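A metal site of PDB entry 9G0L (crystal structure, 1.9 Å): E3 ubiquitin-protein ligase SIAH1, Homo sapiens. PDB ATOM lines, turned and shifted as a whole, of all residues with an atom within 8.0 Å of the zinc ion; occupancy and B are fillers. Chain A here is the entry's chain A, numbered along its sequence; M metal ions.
SG of Cys 36 sits close to N of Asn 38, at 3.6 Å. The side-chain sulfur of Cys 18 sits close to the backbone NH of Asp 20 (3.4 Å). The side-chain sulfur (SG) of Cys 15 sits close to the backbone NH (N) of Val 17 (3.5 Å). The backbone NH of Cys 15 is in hydrogen-bond range of the backbone carbonyl oxygen of Asp 20 (2.7 Å).
Within 4 Å of the zinc ion: Cys 15, Cys 18, Cys 36 and Cys 39.
The zinc ion is bound by the side-chain sulfur (SG) of Cys 36. The side-chain sulfur (SG) of Cys 18 binds the zinc ion (2.3 Å). SG of Cys 39 is bound to the zinc ion (2.3 Å). SG of Cys 15 is bound to the zinc ion, at 2.3 Å.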
ATOM      1  N   PHE A  13     -30.933   6.414 -33.575  1.00  0.00           N
ATOM      2  CA  PHE A  13     -29.793   5.514 -33.651  1.00  0.00           C
ATOM      3  C   PHE A  13     -28.890   5.592 -32.424  1.00  0.00           C
ATOM      4  O   PHE A  13     -27.851   4.945 -32.415  1.00  0.00           O
ATOM      5  CB  PHE A  13     -28.956   5.827 -34.909  1.00  0.00           C
ATOM      6  CG  PHE A  13     -29.668   5.591 -36.223  1.00  0.00           C
ATOM      7  CD1 PHE A  13     -30.576   6.514 -36.709  1.00  0.00           C
ATOM      8  CD2 PHE A  13     -29.392   4.464 -36.981  1.00  0.00           C
ATOM      9  CE1 PHE A  13     -31.226   6.302 -37.929  1.00  0.00           C
ATOM     10  CE2 PHE A  13     -30.019   4.254 -38.198  1.00  0.00           C
ATOM     11  CZ  PHE A  13     -30.931   5.172 -38.677  1.00  0.00           C
ATOM     12  N   GLU A  14     -29.228   6.399 -31.422  1.00  0.00           N
ATOM     13  CA  GLU A  14     -28.339   6.539 -30.270  1.00  0.00           C
ATOM     14  C   GLU A  14     -28.198   5.213 -29.549  1.00  0.00           C
ATOM     15  O   GLU A  14     -29.184   4.528 -29.289  1.00  0.00           O
ATOM     16  CB  GLU A  14     -28.862   7.593 -29.306  1.00  0.00           C
ATOM     17  CG  GLU A  14     -28.268   8.959 -29.525  1.00  0.00           C
ATOM     18  CD  GLU A  14     -28.930   9.990 -28.661  1.00  0.00           C
ATOM     19  OE1 GLU A  14     -29.330   9.631 -27.536  1.00  0.00           O
ATOM     20  OE2 GLU A  14     -29.056  11.150 -29.120  1.00  0.00           O
ATOM     21  N   CYS A  15     -26.960   4.859 -29.232  1.00  0.00           N
ATOM     22  CA  CYS A  15     -26.729   3.693 -28.400  1.00  0.00           C
ATOM     23  C   CYS A  15     -27.185   4.006 -26.982  1.00  0.00           C
ATOM     24  O   CYS A  15     -26.751   5.017 -26.403  1.00  0.00           O
ATOM     25  CB  CYS A  15     -25.248   3.312 -28.414  1.00  0.00           C
ATOM     26  SG  CYS A  15     -24.829   1.937 -27.341  1.00  0.00           S
ATOM     27  N   PRO A  16     -28.067   3.198 -26.376  1.00  0.00           N
ATOM     28  CA  PRO A  16     -28.529   3.512 -25.016  1.00  0.00           C
ATOM     29  C   PRO A  16     -27.458   3.355 -23.958  1.00  0.00           C
ATOM     30  O   PRO A  16     -27.714   3.690 -22.796  1.00  0.00           O
ATOM     31  CB  PRO A  16     -29.683   2.512 -24.804  1.00  0.00           C
ATOM     32  CG  PRO A  16     -29.408   1.387 -25.737  1.00  0.00           C
ATOM     33  CD  PRO A  16     -28.717   2.003 -26.929  1.00  0.00           C
ATOM     34  N   VAL A  17     -26.261   2.906 -24.313  1.00  0.00           N
ATOM     35  CA  VAL A  17     -25.195   2.704 -23.357  1.00  0.00           C
ATOM     36  C   VAL A  17     -24.170   3.830 -23.411  1.00  0.00           C
ATOM     37  O   VAL A  17     -23.805   4.393 -22.381  1.00  0.00           O
ATOM     38  CB  VAL A  17     -24.529   1.333 -23.570  1.00  0.00           C
ATOM     39  CG1 VAL A  17     -23.162   1.295 -22.888  1.00  0.00           C
ATOM     40  CG2 VAL A  17     -25.418   0.231 -23.063  1.00  0.00           C
ATOM     41  N   CYS A  18     -23.691   4.190 -24.611  1.00  0.00           N
ATOM     42  CA  CYS A  18     -22.704   5.261 -24.726  1.00  0.00           C
ATOM     43  C   CYS A  18     -23.263   6.536 -25.355  1.00  0.00           C
ATOM     44  O   CYS A  18     -22.586   7.571 -25.318  1.00  0.00           O
ATOM     45  CB  CYS A  18     -21.504   4.843 -25.588  1.00  0.00           C
ATOM     46  SG  CYS A  18     -21.921   4.475 -27.262  1.00  0.00           S
ATOM     47  N   PHE A  19     -24.443   6.473 -25.953  1.00  0.00           N
ATOM     48  CA  PHE A  19     -25.118   7.585 -26.615  1.00  0.00           C
ATOM     49  C   PHE A  19     -24.363   8.103 -27.837  1.00  0.00           C
ATOM     50  O   PHE A  19     -24.701   9.178 -28.347  1.00  0.00           O
ATOM     51  CB  PHE A  19     -25.420   8.731 -25.644  1.00  0.00           C
ATOM     52  CG  PHE A  19     -26.112   8.277 -24.381  1.00  0.00           C
ATOM     53  CD1 PHE A  19     -25.385   7.875 -23.280  1.00  0.00           C
ATOM     54  CD2 PHE A  19     -27.494   8.209 -24.331  1.00  0.00           C
ATOM     55  CE1 PHE A  19     -26.011   7.436 -22.130  1.00  0.00           C
ATOM     56  CE2 PHE A  19     -28.132   7.762 -23.180  1.00  0.00           C
ATOM     57  CZ  PHE A  19     -27.388   7.384 -22.079  1.00  0.00           C
ATOM     58  N   ASP A  20     -23.350   7.378 -28.318  1.00  0.00           N
ATOM     59  CA  ASP A  20     -22.908   7.537 -29.705  1.00  0.00           C
ATOM     60  C   ASP A  20     -23.938   6.863 -30.604  1.00  0.00           C
ATOM     61  O   ASP A  20     -25.010   6.447 -30.157  1.00  0.00           O
ATOM     62  CB  ASP A  20     -21.520   6.961 -29.923  1.00  0.00           C
ATOM     63  CG  ASP A  20     -20.472   7.604 -29.047  1.00  0.00           C
ATOM     64  OD1 ASP A  20     -20.737   8.701 -28.494  1.00  0.00           O
ATOM     65  OD2 ASP A  20     -19.371   7.021 -28.916  1.00  0.00           O
ATOM     66  N   TYR A  21     -23.622   6.714 -31.885  1.00  0.00           N
ATOM     67  CA  TYR A  21     -24.628   6.280 -32.837  1.00  0.00           C
ATOM     68  C   TYR A  21     -24.391   4.837 -33.238  1.00  0.00           C
ATOM     69  O   TYR A  21     -23.240   4.408 -33.390  1.00  0.00           O
ATOM     70  CB  TYR A  21     -24.645   7.198 -34.061  1.00  0.00           C
ATOM     71  CG  TYR A  21     -25.107   8.579 -33.690  1.00  0.00           C
ATOM     72  CD1 TYR A  21     -26.452   8.836 -33.461  1.00  0.00           C
ATOM     73  CD2 TYR A  21     -24.211   9.620 -33.528  1.00  0.00           C
ATOM     74  CE1 TYR A  21     -26.896  10.086 -33.102  1.00  0.00           C
ATOM     75  CE2 TYR A  21     -24.653  10.894 -33.165  1.00  0.00           C
ATOM     76  CZ  TYR A  21     -26.002  11.116 -32.949  1.00  0.00           C
ATOM     77  OH  TYR A  21     -26.465  12.355 -32.595  1.00  0.00           O
ATOM     78  N   VAL A  22     -25.480   4.085 -33.385  1.00  0.00           N
ATOM     79  CA  VAL A  22     -25.442   2.711 -33.873  1.00  0.00           C
ATOM     80  C   VAL A  22     -25.488   2.779 -35.388  1.00  0.00           C
ATOM     81  O   VAL A  22     -26.510   3.145 -35.975  1.00  0.00           O
ATOM     82  CB  VAL A  22     -26.600   1.877 -33.318  1.00  0.00           C
ATOM     83  CG1 VAL A  22     -26.468   0.431 -33.772  1.00  0.00           C
ATOM     84  CG2 VAL A  22     -26.626   1.944 -31.795  1.00  0.00           C
ATOM     85  N   LEU A  34     -31.314  -1.602 -29.577  1.00  0.00           N
ATOM     86  CA  LEU A  34     -30.088  -1.459 -30.335  1.00  0.00           C
ATOM     87  C   LEU A  34     -28.907  -1.297 -29.370  1.00  0.00           C
ATOM     88  O   LEU A  34     -29.071  -0.775 -28.269  1.00  0.00           O
ATOM     89  CB  LEU A  34     -30.171  -0.234 -31.252  1.00  0.00           C
ATOM     90  CG  LEU A  34     -31.297  -0.068 -32.298  1.00  0.00           C
ATOM     91  CD1 LEU A  34     -30.882   0.988 -33.301  1.00  0.00           C
ATOM     92  CD2 LEU A  34     -31.609  -1.334 -33.033  1.00  0.00           C
ATOM     93  N   VAL A  35     -27.729  -1.763 -29.790  1.00  0.00           N
ATOM     94  CA  VAL A  35     -26.461  -1.500 -29.096  1.00  0.00           C
ATOM     95  C   VAL A  35     -25.385  -1.314 -30.161  1.00  0.00           C
ATOM     96  O   VAL A  35     -25.369  -2.047 -31.158  1.00  0.00           O
ATOM     97  CB  VAL A  35     -26.013  -2.644 -28.159  1.00  0.00           C
ATOM     98  CG1 VAL A  35     -25.009  -2.133 -27.143  1.00  0.00           C
ATOM     99  CG2 VAL A  35     -27.190  -3.293 -27.488  1.00  0.00           C
ATOM    100  N   CYS A  36     -24.478  -0.370 -29.937  1.00  0.00           N
ATOM    101  CA  CYS A  36     -23.483  -0.071 -30.974  1.00  0.00           C
ATOM    102  C   CYS A  36     -22.385  -1.133 -31.010  1.00  0.00           C
ATOM    103  O   CYS A  36     -22.264  -1.972 -30.116  1.00  0.00           O
ATOM    104  CB  CYS A  36     -22.868   1.306 -30.779  1.00  0.00           C
ATOM    105  SG  CYS A  36     -21.689   1.448 -29.422  1.00  0.00           S
ATOM    106  N   SER A  37     -21.576  -1.057 -32.068  1.00  0.00           N
ATOM    107  CA  SER A  37     -20.542  -2.062 -32.309  1.00  0.00           C
ATOM    108  C   SER A  37     -19.526  -2.090 -31.181  1.00  0.00           C
ATOM    109  O   SER A  37     -18.990  -3.155 -30.855  1.00  0.00           O
ATOM    110  CB  SER A  37     -19.836  -1.766 -33.631  1.00  0.00           C
ATOM    111  OG  SER A  37     -20.614  -2.205 -34.731  1.00  0.00           O
ATOM    112  N   ASN A  38     -19.263  -0.944 -30.559  1.00  0.00           N
ATOM    113  CA  ASN A  38     -18.211  -0.864 -29.552  1.00  0.00           C
ATOM    114  C   ASN A  38     -18.692  -1.325 -28.179  1.00  0.00           C
ATOM    115  O   ASN A  38     -17.895  -1.878 -27.410  1.00  0.00           O
ATOM    116  CB  ASN A  38     -17.688   0.572 -29.467  1.00  0.00           C
ATOM    117  CG  ASN A  38     -17.250   1.112 -30.825  1.00  0.00           C
ATOM    118  OD1 ASN A  38     -16.601   0.417 -31.616  1.00  0.00           O
ATOM    119  ND2 ASN A  38     -17.608   2.363 -31.105  1.00  0.00           N
ATOM    120  N   CYS A  39     -19.966  -1.098 -27.861  1.00  0.00           N
ATOM    121  CA  CYS A  39     -20.486  -1.524 -26.569  1.00  0.00           C
ATOM    122  C   CYS A  39     -20.803  -3.014 -26.566  1.00  0.00           C
ATOM    123  O   CYS A  39     -20.584  -3.691 -25.554  1.00  0.00           O
ATOM    124  CB  CYS A  39     -21.745  -0.730 -26.231  1.00  0.00           C
ATOM    125  SG  CYS A  39     -21.402   0.971 -25.816  1.00  0.00           S
ATOM    126  N   ARG A  40     -21.330  -3.524 -27.671  1.00  0.00           N
ATOM    127  CA  ARG A  40     -21.705  -4.935 -27.811  1.00  0.00           C
ATOM    128  C   ARG A  40     -20.714  -5.914 -27.205  1.00  0.00           C
ATOM    129  O   ARG A  40     -21.140  -6.778 -26.416  1.00  0.00           O
ATOM    130  CB  ARG A  40     -21.929  -5.209 -29.303  1.00  0.00           C
ATOM    131  CG  ARG A  40     -22.775  -6.396 -29.603  1.00  0.00           C
ATOM    132  CD  ARG A  40     -23.327  -6.270 -31.005  1.00  0.00           C
ATOM    133  NE  ARG A  40     -24.538  -5.479 -31.006  1.00  0.00           N
ATOM    134  CZ  ARG A  40     -25.748  -5.999 -30.877  1.00  0.00           C
ATOM    135  NH1 ARG A  40     -25.922  -7.303 -30.740  1.00  0.00           N
ATOM    136  NH2 ARG A  40     -26.814  -5.193 -30.861  1.00  0.00           N
ATOM    137  N   LEU A  43     -20.653  -6.568 -23.246  1.00  0.00           N
ATOM    138  CA  LEU A  43     -21.949  -6.873 -22.669  1.00  0.00           C
ATOM    139  C   LEU A  43     -22.281  -8.346 -22.879  1.00  0.00           C
ATOM    140  O   LEU A  43     -21.876  -8.948 -23.890  1.00  0.00           O
ATOM    141  CB  LEU A  43     -23.041  -6.014 -23.297  1.00  0.00           C
ATOM    142  CG  LEU A  43     -23.044  -4.536 -22.879  1.00  0.00           C
ATOM    143  CD1 LEU A  43     -23.955  -3.743 -23.797  1.00  0.00           C
ATOM    144  CD2 LEU A  43     -23.417  -4.367 -21.415  1.00  0.00           C
ATOM    145  N   PRO A  47     -28.687  -4.413 -22.978  1.00  0.00           N
ATOM    146  CA  PRO A  47     -28.702  -3.507 -21.820  1.00  0.00           C
ATOM    147  C   PRO A  47     -30.069  -2.973 -21.497  1.00  0.00           C
ATOM    148  O   PRO A  47     -30.300  -2.514 -20.371  1.00  0.00           O
ATOM    149  CB  PRO A  47     -27.756  -2.373 -22.231  1.00  0.00           C
ATOM    150  CG  PRO A  47     -27.402  -2.600 -23.665  1.00  0.00           C
ATOM    151  CD  PRO A  47     -28.200  -3.749 -24.194  1.00  0.00           C
HETATM  152 ZN    ZN M   1     -22.507   2.240 -27.433  1.00  0.00          ZN
